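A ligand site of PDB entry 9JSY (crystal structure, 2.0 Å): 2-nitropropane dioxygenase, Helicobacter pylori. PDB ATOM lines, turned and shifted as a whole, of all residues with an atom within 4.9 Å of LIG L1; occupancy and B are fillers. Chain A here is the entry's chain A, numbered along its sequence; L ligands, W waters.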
ATOM      1  N   GLY A  24      30.152  18.945 -18.283  1.00  0.00           N
ATOM      2  CA  GLY A  24      29.034  19.453 -17.509  1.00  0.00           C
ATOM      3  C   GLY A  24      27.724  19.212 -18.242  1.00  0.00           C
ATOM      4  O   GLY A  24      27.661  19.266 -19.473  1.00  0.00           O
ATOM      5  N   GLY A  25      26.677  18.897 -17.478  1.00  0.00           N
ATOM      6  CA  GLY A  25      25.356  18.758 -18.074  1.00  0.00           C
ATOM      7  C   GLY A  25      24.895  20.066 -18.687  1.00  0.00           C
ATOM      8  O   GLY A  25      25.170  21.148 -18.158  1.00  0.00           O
ATOM      9  N   MET A  26      24.212  19.977 -19.832  1.00  0.00           N
ATOM     10  CA  MET A  26      23.746  21.191 -20.491  1.00  0.00           C
ATOM     11  C   MET A  26      22.374  20.934 -21.097  1.00  0.00           C
ATOM     12  O   MET A  26      22.227  20.093 -21.998  1.00  0.00           O
ATOM     13  CB  MET A  26      24.740  21.657 -21.579  1.00  0.00           C
ATOM     14  CG  MET A  26      26.079  22.273 -21.063  1.00  0.00           C
ATOM     15  SD  MET A  26      27.250  22.666 -22.400  1.00  0.00           S
ATOM     16  CE  MET A  26      28.060  21.089 -22.685  1.00  0.00           C
ATOM     17  N   GLY A  27      21.371  21.653 -20.628  1.00  0.00           N
ATOM     18  CA  GLY A  27      20.051  21.606 -21.233  1.00  0.00           C
ATOM     19  C   GLY A  27      19.765  22.870 -22.017  1.00  0.00           C
ATOM     20  O   GLY A  27      20.482  23.863 -21.918  1.00  0.00           O
ATOM     21  N   ILE A  30      21.361  19.711 -25.137  1.00  0.00           N
ATOM     22  CA  ILE A  30      22.734  19.909 -25.566  1.00  0.00           C
ATOM     23  C   ILE A  30      23.608  18.712 -25.229  1.00  0.00           C
ATOM     24  O   ILE A  30      24.369  18.241 -26.061  1.00  0.00           O
ATOM     25  CB  ILE A  30      23.278  21.232 -24.981  1.00  0.00           C
ATOM     26  CG1 ILE A  30      22.338  22.382 -25.389  1.00  0.00           C
ATOM     27  CG2 ILE A  30      24.791  21.377 -25.234  1.00  0.00           C
ATOM     28  CD1 ILE A  30      22.541  23.672 -24.665  1.00  0.00           C
ATOM     29  N   SER A  49      21.696  15.670 -19.565  1.00  0.00           N
ATOM     30  CA  SER A  49      20.775  16.602 -18.925  1.00  0.00           C
ATOM     31  C   SER A  49      19.375  15.996 -18.940  1.00  0.00           C
ATOM     32  O   SER A  49      18.890  15.548 -19.984  1.00  0.00           O
ATOM     33  CB  SER A  49      20.792  17.953 -19.642  1.00  0.00           C
ATOM     34  OG  SER A  49      19.648  18.739 -19.305  1.00  0.00           O
ATOM     35  N   VAL A  51      16.594  17.608 -18.094  1.00  0.00           N
ATOM     36  CA  VAL A  51      15.568  18.646 -18.194  1.00  0.00           C
ATOM     37  C   VAL A  51      15.097  18.773 -19.645  1.00  0.00           C
ATOM     38  O   VAL A  51      15.877  18.673 -20.591  1.00  0.00           O
ATOM     39  CB  VAL A  51      16.066  19.994 -17.622  1.00  0.00           C
ATOM     40  CG1 VAL A  51      16.631  19.779 -16.227  1.00  0.00           C
ATOM     41  CG2 VAL A  51      17.131  20.600 -18.520  1.00  0.00           C
ATOM     42  N   ASN A 101      22.115  15.120 -14.977  1.00  0.00           N
ATOM     43  CA  ASN A 101      22.080  16.422 -14.329  1.00  0.00           C
ATOM     44  C   ASN A 101      20.624  16.858 -14.182  1.00  0.00           C
ATOM     45  O   ASN A 101      19.871  16.879 -15.166  1.00  0.00           O
ATOM     46  CB  ASN A 101      22.884  17.444 -15.141  1.00  0.00           C
ATOM     47  CG  ASN A 101      22.855  18.822 -14.523  1.00  0.00           C
ATOM     48  OD1 ASN A 101      21.794  19.444 -14.404  1.00  0.00           O
ATOM     49  ND2 ASN A 101      24.016  19.306 -14.082  1.00  0.00           N
ATOM     50  N   LEU A 103      18.442  19.976 -12.296  1.00  0.00           N
ATOM     51  CA  LEU A 103      18.342  21.189 -11.500  1.00  0.00           C
ATOM     52  C   LEU A 103      17.299  21.027 -10.398  1.00  0.00           C
ATOM     53  O   LEU A 103      16.185  20.529 -10.624  1.00  0.00           O
ATOM     54  CB  LEU A 103      18.005  22.408 -12.371  1.00  0.00           C
ATOM     55  CG  LEU A 103      18.971  22.645 -13.541  1.00  0.00           C
ATOM     56  CD1 LEU A 103      18.337  23.252 -14.758  1.00  0.00           C
ATOM     57  CD2 LEU A 103      20.117  23.510 -13.002  1.00  0.00           C
ATOM     58  N   GLY A 127      22.318  21.110  -9.096  1.00  0.00           N
ATOM     59  CA  GLY A 127      22.511  22.478  -8.620  1.00  0.00           C
ATOM     60  C   GLY A 127      21.226  23.283  -8.634  1.00  0.00           C
ATOM     61  O   GLY A 127      20.147  22.688  -8.565  1.00  0.00           O
ATOM     62  N   ILE A 149      25.920  20.524  -6.627  1.00  0.00           N
ATOM     63  CA  ILE A 149      26.695  21.685  -7.069  1.00  0.00           C
ATOM     64  C   ILE A 149      26.515  22.773  -6.020  1.00  0.00           C
ATOM     65  O   ILE A 149      25.384  23.086  -5.636  1.00  0.00           O
ATOM     66  CB  ILE A 149      26.249  22.175  -8.453  1.00  0.00           C
ATOM     67  CG1 ILE A 149      26.139  21.026  -9.467  1.00  0.00           C
ATOM     68  CG2 ILE A 149      27.205  23.251  -8.996  1.00  0.00           C
ATOM     69  CD1 ILE A 149      25.874  21.494 -10.900  1.00  0.00           C
ATOM     70  N   GLU A 177      31.053  25.535  -8.218  1.00  0.00           N
ATOM     71  CA  GLU A 177      30.910  26.456  -9.330  1.00  0.00           C
ATOM     72  C   GLU A 177      30.621  27.833  -8.755  1.00  0.00           C
ATOM     73  O   GLU A 177      29.638  28.004  -8.013  1.00  0.00           O
ATOM     74  CB  GLU A 177      29.799  26.006 -10.291  1.00  0.00           C
ATOM     75  CG  GLU A 177      29.604  26.886 -11.520  1.00  0.00           C
ATOM     76  CD  GLU A 177      28.284  26.612 -12.229  1.00  0.00           C
ATOM     77  OE1 GLU A 177      27.225  26.752 -11.590  1.00  0.00           O
ATOM     78  OE2 GLU A 177      28.307  26.242 -13.425  1.00  0.00           O
ATOM     79  N   ALA A 221      34.553  23.819 -11.198  1.00  0.00           N
ATOM     80  CA  ALA A 221      33.817  24.099 -12.428  1.00  0.00           C
ATOM     81  C   ALA A 221      33.678  25.598 -12.667  1.00  0.00           C
ATOM     82  O   ALA A 221      33.490  26.369 -11.725  1.00  0.00           O
ATOM     83  CB  ALA A 221      32.422  23.456 -12.404  1.00  0.00           C
ATOM     84  N   GLY A 222      33.754  25.985 -13.937  1.00  0.00           N
ATOM     85  CA  GLY A 222      33.502  27.361 -14.324  1.00  0.00           C
ATOM     86  C   GLY A 222      34.752  28.059 -14.812  1.00  0.00           C
ATOM     87  O   GLY A 222      35.621  28.404 -14.018  1.00  0.00           O
ATOM     88  N   GLY A 223      34.848  28.280 -16.129  1.00  0.00           N
ATOM     89  CA  GLY A 223      35.993  28.993 -16.680  1.00  0.00           C
ATOM     90  C   GLY A 223      37.232  28.154 -16.897  1.00  0.00           C
ATOM     91  O   GLY A 223      38.292  28.711 -17.189  1.00  0.00           O
ATOM     92  N   ILE A 224      37.137  26.843 -16.762  1.00  0.00           N
ATOM     93  CA  ILE A 224      38.269  25.950 -16.989  1.00  0.00           C
ATOM     94  C   ILE A 224      38.321  25.630 -18.467  1.00  0.00           C
ATOM     95  O   ILE A 224      37.384  25.040 -19.018  1.00  0.00           O
ATOM     96  CB  ILE A 224      38.161  24.683 -16.122  1.00  0.00           C
ATOM     97  CG1 ILE A 224      38.120  25.104 -14.649  1.00  0.00           C
ATOM     98  CG2 ILE A 224      39.298  23.681 -16.436  1.00  0.00           C
ATOM     99  CD1 ILE A 224      37.815  23.998 -13.707  1.00  0.00           C
ATOM    100  N   GLN A 242      35.028  20.034 -13.886  1.00  0.00           N
ATOM    101  CA  GLN A 242      33.857  19.946 -14.744  1.00  0.00           C
ATOM    102  C   GLN A 242      33.971  21.055 -15.779  1.00  0.00           C
ATOM    103  O   GLN A 242      34.269  22.214 -15.434  1.00  0.00           O
ATOM    104  CB  GLN A 242      32.544  20.098 -13.963  1.00  0.00           C
ATOM    105  CG  GLN A 242      31.352  20.195 -14.899  1.00  0.00           C
ATOM    106  CD  GLN A 242      30.029  20.096 -14.197  1.00  0.00           C
ATOM    107  OE1 GLN A 242      29.556  18.997 -13.860  1.00  0.00           O
ATOM    108  NE2 GLN A 242      29.412  21.240 -13.992  1.00  0.00           N
ATOM    109  N   MET A 243      33.765  20.707 -17.047  1.00  0.00           N
ATOM    110  CA  MET A 243      33.926  21.633 -18.154  1.00  0.00           C
ATOM    111  C   MET A 243      32.694  21.491 -19.039  1.00  0.00           C
ATOM    112  O   MET A 243      32.310  20.364 -19.366  1.00  0.00           O
ATOM    113  CB  MET A 243      35.185  21.279 -18.926  1.00  0.00           C
ATOM    114  CG  MET A 243      36.464  21.620 -18.169  1.00  0.00           C
ATOM    115  SD  MET A 243      37.896  20.859 -18.981  1.00  0.00           S
ATOM    116  CE  MET A 243      38.363  22.167 -20.108  1.00  0.00           C
ATOM    117  N   ALA A 244      32.060  22.608 -19.394  1.00  0.00           N
ATOM    118  CA  ALA A 244      30.930  22.537 -20.311  1.00  0.00           C
ATOM    119  C   ALA A 244      31.189  23.256 -21.626  1.00  0.00           C
ATOM    120  O   ALA A 244      31.024  22.644 -22.704  1.00  0.00           O
ATOM    121  CB  ALA A 244      29.653  23.091 -19.656  1.00  0.00           C
ATOM    122  N   THR A 245      31.604  24.525 -21.589  1.00  0.00           N
ATOM    123  CA  THR A 245      31.766  25.305 -22.810  1.00  0.00           C
ATOM    124  C   THR A 245      32.666  24.625 -23.848  1.00  0.00           C
ATOM    125  O   THR A 245      32.359  24.666 -25.044  1.00  0.00           O
ATOM    126  CB  THR A 245      32.281  26.723 -22.509  1.00  0.00           C
ATOM    127  OG1 THR A 245      31.287  27.465 -21.790  1.00  0.00           O
ATOM    128  CG2 THR A 245      32.592  27.478 -23.813  1.00  0.00           C
ATOM    129  N   LEU A 248      30.620  22.100 -25.588  1.00  0.00           N
ATOM    130  CA  LEU A 248      29.657  22.800 -26.433  1.00  0.00           C
ATOM    131  C   LEU A 248      30.241  23.067 -27.819  1.00  0.00           C
ATOM    132  O   LEU A 248      29.493  23.197 -28.786  1.00  0.00           O
ATOM    133  CB  LEU A 248      29.282  24.126 -25.765  1.00  0.00           C
ATOM    134  CG  LEU A 248      28.117  24.971 -26.222  1.00  0.00           C
ATOM    135  CD1 LEU A 248      26.813  24.182 -26.061  1.00  0.00           C
ATOM    136  CD2 LEU A 248      28.090  26.258 -25.404  1.00  0.00           C
ATOM    137  N   TYR A 258      24.801  24.972 -32.216  1.00  0.00           N
ATOM    138  CA  TYR A 258      25.977  25.594 -31.614  1.00  0.00           C
ATOM    139  C   TYR A 258      27.215  25.440 -32.493  1.00  0.00           C
ATOM    140  O   TYR A 258      28.074  26.331 -32.510  1.00  0.00           O
ATOM    141  CB  TYR A 258      26.233  25.010 -30.220  1.00  0.00           C
ATOM    142  CG  TYR A 258      25.297  25.588 -29.165  1.00  0.00           C
ATOM    143  CD1 TYR A 258      25.611  26.769 -28.494  1.00  0.00           C
ATOM    144  CD2 TYR A 258      24.113  24.931 -28.842  1.00  0.00           C
ATOM    145  CE1 TYR A 258      24.756  27.288 -27.548  1.00  0.00           C
ATOM    146  CE2 TYR A 258      23.260  25.438 -27.876  1.00  0.00           C
ATOM    147  CZ  TYR A 258      23.596  26.622 -27.239  1.00  0.00           C
ATOM    148  OH  TYR A 258      22.752  27.108 -26.273  1.00  0.00           O
ATOM    149  N   PHE A 341      22.714  29.567 -24.551  1.00  0.00           N
ATOM    150  CA  PHE A 341      23.586  29.769 -23.404  1.00  0.00           C
ATOM    151  C   PHE A 341      25.057  29.547 -23.771  1.00  0.00           C
ATOM    152  O   PHE A 341      25.386  28.811 -24.716  1.00  0.00           O
ATOM    153  CB  PHE A 341      23.217  28.801 -22.285  1.00  0.00           C
ATOM    154  CG  PHE A 341      21.962  29.165 -21.521  1.00  0.00           C
ATOM    155  CD1 PHE A 341      21.346  30.396 -21.696  1.00  0.00           C
ATOM    156  CD2 PHE A 341      21.405  28.260 -20.624  1.00  0.00           C
ATOM    157  CE1 PHE A 341      20.212  30.728 -20.961  1.00  0.00           C
ATOM    158  CE2 PHE A 341      20.264  28.575 -19.904  1.00  0.00           C
ATOM    159  CZ  PHE A 341      19.668  29.814 -20.071  1.00  0.00           C
ATOM    160  N   THR A 342      25.944  30.156 -22.990  1.00  0.00           N
ATOM    161  CA  THR A 342      27.381  29.911 -23.117  1.00  0.00           C
ATOM    162  C   THR A 342      28.061  30.291 -21.808  1.00  0.00           C
ATOM    163  O   THR A 342      27.609  31.189 -21.094  1.00  0.00           O
ATOM    164  CB  THR A 342      27.997  30.710 -24.274  1.00  0.00           C
ATOM    165  OG1 THR A 342      29.403  30.409 -24.355  1.00  0.00           O
ATOM    166  CG2 THR A 342      27.809  32.210 -24.084  1.00  0.00           C
ATOM    167  N   GLY A 343      29.161  29.603 -21.499  1.00  0.00           N
ATOM    168  CA  GLY A 343      30.050  30.092 -20.457  1.00  0.00           C
ATOM    169  C   GLY A 343      30.748  31.351 -20.922  1.00  0.00           C
ATOM    170  O   GLY A 343      30.699  31.740 -22.095  1.00  0.00           O
HETATM  171  N1  LIG L   1      24.399  23.457 -15.380  1.00  0.00           N
HETATM  172  C1  LIG L   1      23.469  22.581 -14.759  1.00  0.00           C
HETATM  173  O1  LIG L   1      23.638  22.198 -13.600  1.00  0.00           O
HETATM  174  N2  LIG L   1      22.384  22.123 -15.469  1.00  0.00           N
HETATM  175  C2  LIG L   1      22.197  22.532 -16.800  1.00  0.00           C
HETATM  176  O2  LIG L   1      21.214  22.116 -17.418  1.00  0.00           O
HETATM  177  C3  LIG L   1      23.121  23.405 -17.402  1.00  0.00           C
HETATM  178  N3  LIG L   1      22.957  23.805 -18.674  1.00  0.00           N
HETATM  179  C4  LIG L   1      23.914  24.518 -19.297  1.00  0.00           C
HETATM  180  C5  LIG L   1      23.799  24.797 -20.664  1.00  0.00           C
HETATM  181  C6  LIG L   1      24.793  25.505 -21.339  1.00  0.00           C
HETATM  182  C7  LIG L   1      24.656  25.766 -22.706  1.00  0.00           C
HETATM  183  C8  LIG L   1      25.925  25.954 -20.648  1.00  0.00           C
HETATM  184  C9  LIG L   1      26.940  26.690 -21.312  1.00  0.00           C
HETATM  185  C10 LIG L   1      26.031  25.685 -19.282  1.00  0.00           C
HETATM  186  C11 LIG L   1      25.031  24.984 -18.587  1.00  0.00           C
HETATM  187  N4  LIG L   1      25.150  24.682 -17.274  1.00  0.00           N
HETATM  188  C12 LIG L   1      24.229  23.883 -16.693  1.00  0.00           C
HETATM  189  C13 LIG L   1      26.420  24.965 -16.538  1.00  0.00           C
HETATM  190  C14 LIG L   1      27.464  23.886 -16.913  1.00  0.00           C
HETATM  191  O3  LIG L   1      27.015  22.550 -16.558  1.00  0.00           O
HETATM  192  C15 LIG L   1      28.866  24.107 -16.281  1.00  0.00           C
HETATM  193  O4  LIG L   1      28.853  23.847 -14.868  1.00  0.00           O
HETATM  194  C16 LIG L   1      29.461  25.508 -16.507  1.00  0.00           C
HETATM  195  O5  LIG L   1      29.027  26.154 -17.717  1.00  0.00           O
HETATM  196  C17 LIG L   1      30.952  25.213 -16.591  1.00  0.00           C
HETATM  197  O6  LIG L   1      31.623  26.364 -17.005  1.00  0.00           O
HETATM  198  P1  LIG L   1      32.324  26.414 -18.392  1.00  0.00           P
HETATM  199  O7  LIG L   1      33.106  25.154 -18.421  1.00  0.00           O
HETATM  200  O8  LIG L   1      31.231  26.484 -19.385  1.00  0.00           O
HETATM  201  O9  LIG L   1      33.125  27.625 -18.227  1.00  0.00           O
HETATM  202  C1  LG2 L   2      23.591  28.678 -17.623  1.00  0.00           C
HETATM  203  C2  LG2 L   2      26.265  29.350 -17.185  1.00  0.00           C
HETATM  204  C3  LG2 L   2      21.092  29.215 -14.739  1.00  0.00           C
HETATM  205  C4  LG2 L   2      20.056  30.143 -14.572  1.00  0.00           C
HETATM  206  C5  LG2 L   2      15.529  25.729 -16.731  1.00  0.00           C
HETATM  207  C6  LG2 L   2      17.892  24.983 -17.959  1.00  0.00           C
HETATM  208  C7  LG2 L   2      17.913  25.923 -16.927  1.00  0.00           C
HETATM  209  C8  LG2 L   2      19.447  27.771 -15.846  1.00  0.00           C
HETATM  210  C9  LG2 L   2      20.755  28.021 -15.377  1.00  0.00           C
HETATM  211  C10 LG2 L   2      24.229  28.280 -16.451  1.00  0.00           C
HETATM  212  C11 LG2 L   2      24.297  29.412 -18.579  1.00  0.00           C
HETATM  213  C12 LG2 L   2      25.641  29.768 -18.360  1.00  0.00           C
HETATM  214  C13 LG2 L   2      27.746  29.696 -16.870  1.00  0.00           C
HETATM  215  C14 LG2 L   2      29.799  29.184 -15.752  1.00  0.00           C
HETATM  216  C15 LG2 L   2      25.566  28.619 -16.248  1.00  0.00           C
HETATM  217  C16 LG2 L   2      18.772  29.825 -15.073  1.00  0.00           C
HETATM  218  C17 LG2 L   2      16.735  26.294 -16.307  1.00  0.00           C
HETATM  219  C18 LG2 L   2      15.530  24.789 -17.766  1.00  0.00           C
HETATM  220  C19 LG2 L   2      16.696  24.407 -18.381  1.00  0.00           C
HETATM  221  N1  LG2 L   2      19.222  26.477 -16.535  1.00  0.00           N
HETATM  222  N2  LG2 L   2      23.561  27.499 -15.394  1.00  0.00           N
HETATM  223  N3  LG2 L   2      18.507  28.666 -15.694  1.00  0.00           N
HETATM  224  O1  LG2 L   2      28.391  29.010 -15.809  1.00  0.00           O
HETATM  225  O2  LG2 L   2      28.313  30.528 -17.487  1.00  0.00           O
HETATM  226  O3  LG2 L   2      21.887  25.610 -14.724  1.00  0.00           O
HETATM  227  O4  LG2 L   2      21.918  26.132 -16.955  1.00  0.00           O
HETATM  228  S1  LG2 L   2      22.026  26.740 -15.632  1.00  0.00           S
HETATM  229 CL1  LG2 L   2      19.404  24.488 -18.742  1.00  0.00          CL
HETATM  230 CL2  LG2 L   2      13.987  24.074 -18.298  1.00  0.00          CL
HETATM  231  O   HOH W   1      34.691  24.795 -16.396  1.00  0.00           O
HETATM  232  O   HOH W   2      35.417  27.522 -19.806  1.00  0.00           O
HETATM  233  O   HOH W   3      20.190  19.678 -17.013  1.00  0.00           O
HETATM  234  O   HOH W   4      21.686  20.923 -11.848  1.00  0.00           O
HETATM  235  O   HOH W   5      26.561  21.637 -14.071  1.00  0.00           O
HETATM  236  O   HOH W   6      34.805  24.540 -20.515  1.00  0.00           O
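The backbone NH of Ala 244 is in hydrogen-bond range of an oxygen (O7) of LIG L1. An oxygen (O8) of LIG L1 lies within hydrogen-bond range of the side-chain hydroxyl (OG1) of Thr 245 (2.6 Å). The side-chain carboxylate of Glu 177 is in hydrogen-bond range of an oxygen (O4) of LIG L1, 2.8 Å away. The backbone NH (N) of Gly 27 sits at hydrogen-bond distance from an oxygen (O2) of LIG L1, at 3.2 Å. The backbone carbonyl oxygen (O) of Gly 25 lies within hydrogen-bond range of an oxygen (O3) of LIG L1, at 2.8 Å. The side-chain amide nitrogen (NE2) of Gln 242 is in hydrogen-bond range of an oxygen (O4) of LIG L1 (2.8 Å). The side-chain amide oxygen (OD1) of Asn 101 is in hydrogen-bond range of a nitrogen (N2) of LIG L1 (2.9 Å). N of Gly 223 lies within hydrogen-bond range of O9 of LIG L1 (2.8 Å). O8 of LIG L1 is in hydrogen-bond range of N of Thr 245 (3.0 Å).
O5 of LIG L1 lies within hydrogen-bond range of O1 of LG2 L2, at 3.5 Å.
OG1 of Thr 245 lies within hydrogen-bond range of N of Gly 343 (3.0 Å). The backbone NH (N) of Gly 24 sits at hydrogen-bond distance from the backbone carbonyl oxygen (O) of Met 243 (2.8 Å). The backbone NH of Phe 341 is in hydrogen-bond range of the side-chain hydroxyl of Tyr 258 (3.0 Å).
Gly 24 touches LIG L1 (C to O3, 3.8 Å). Met 26 touches LIG L1. CD1 of Ile 30 touches C7 of LIG L1, 3.6 Å away. Leu 103 touches LIG L1 (CD2 to N2, 3.6 Å). Ile 149 touches LIG L1 (CD1 to O1, 3.6 Å). Gly 222 touches LIG L1. Met 243 touches LIG L1. Phe 341 touches LIG L1 (CB to C7, 3.4 Å). Thr 342 touches LIG L1. N of Gly 343 touches C9 of LIG L1, 3.7 Å away. Hydrophobic or aromatic side chains that line LIG L1: Met 26, Ile 30, Leu 103, Ile 149, Ala 244 and Phe 341. Within 4 Å of LIG L1: Gly 24, Gly 25, Met 26, Gly 27, Ile 30, Asn 101, Leu 103, Ile 149, Glu 177, Gly 222, Gly 223, Gln 242, Met 243, Ala 244, Thr 245, Phe 341, Thr 342 and Gly 343. Along chain A the residues within 4 Å of LIG L1 span positions 24 to 343. The nearest printed residue that does not touch LIG L1 is Ser 49 (4.2 Å).
Water W3 lies within hydrogen-bond range of OG of Ser 49 (2.5 Å), O2 of LIG L1 (2.7 Å) and OD1 of Asn 101 (3.1 Å). Water W5 lies within hydrogen-bond range of an oxygen (O3) of LIG L1 (2.7 Å), the side-chain amide nitrogen (NE2) of Gln 242 (2.9 Å) and the side-chain amide nitrogen (ND2) of Asn 101 (3.5 Å). Water W6 lies within hydrogen-bond range of O7 of LIG L1, O of Ile 224 and N of Thr 245. Water W2 bridges an oxygen (O9) of LIG L1 (2.8 Å) and the backbone carbonyl oxygen of Ile 224 (3.3 Å). Water W4 lies within hydrogen-bond range of the backbone NH of Gly 127 (2.8 Å), an oxygen (O1) of LIG L1 (2.9 Å), the side-chain amide oxygen of Asn 101 (3.0 Å) and the backbone NH of Leu 103 (3.4 Å).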
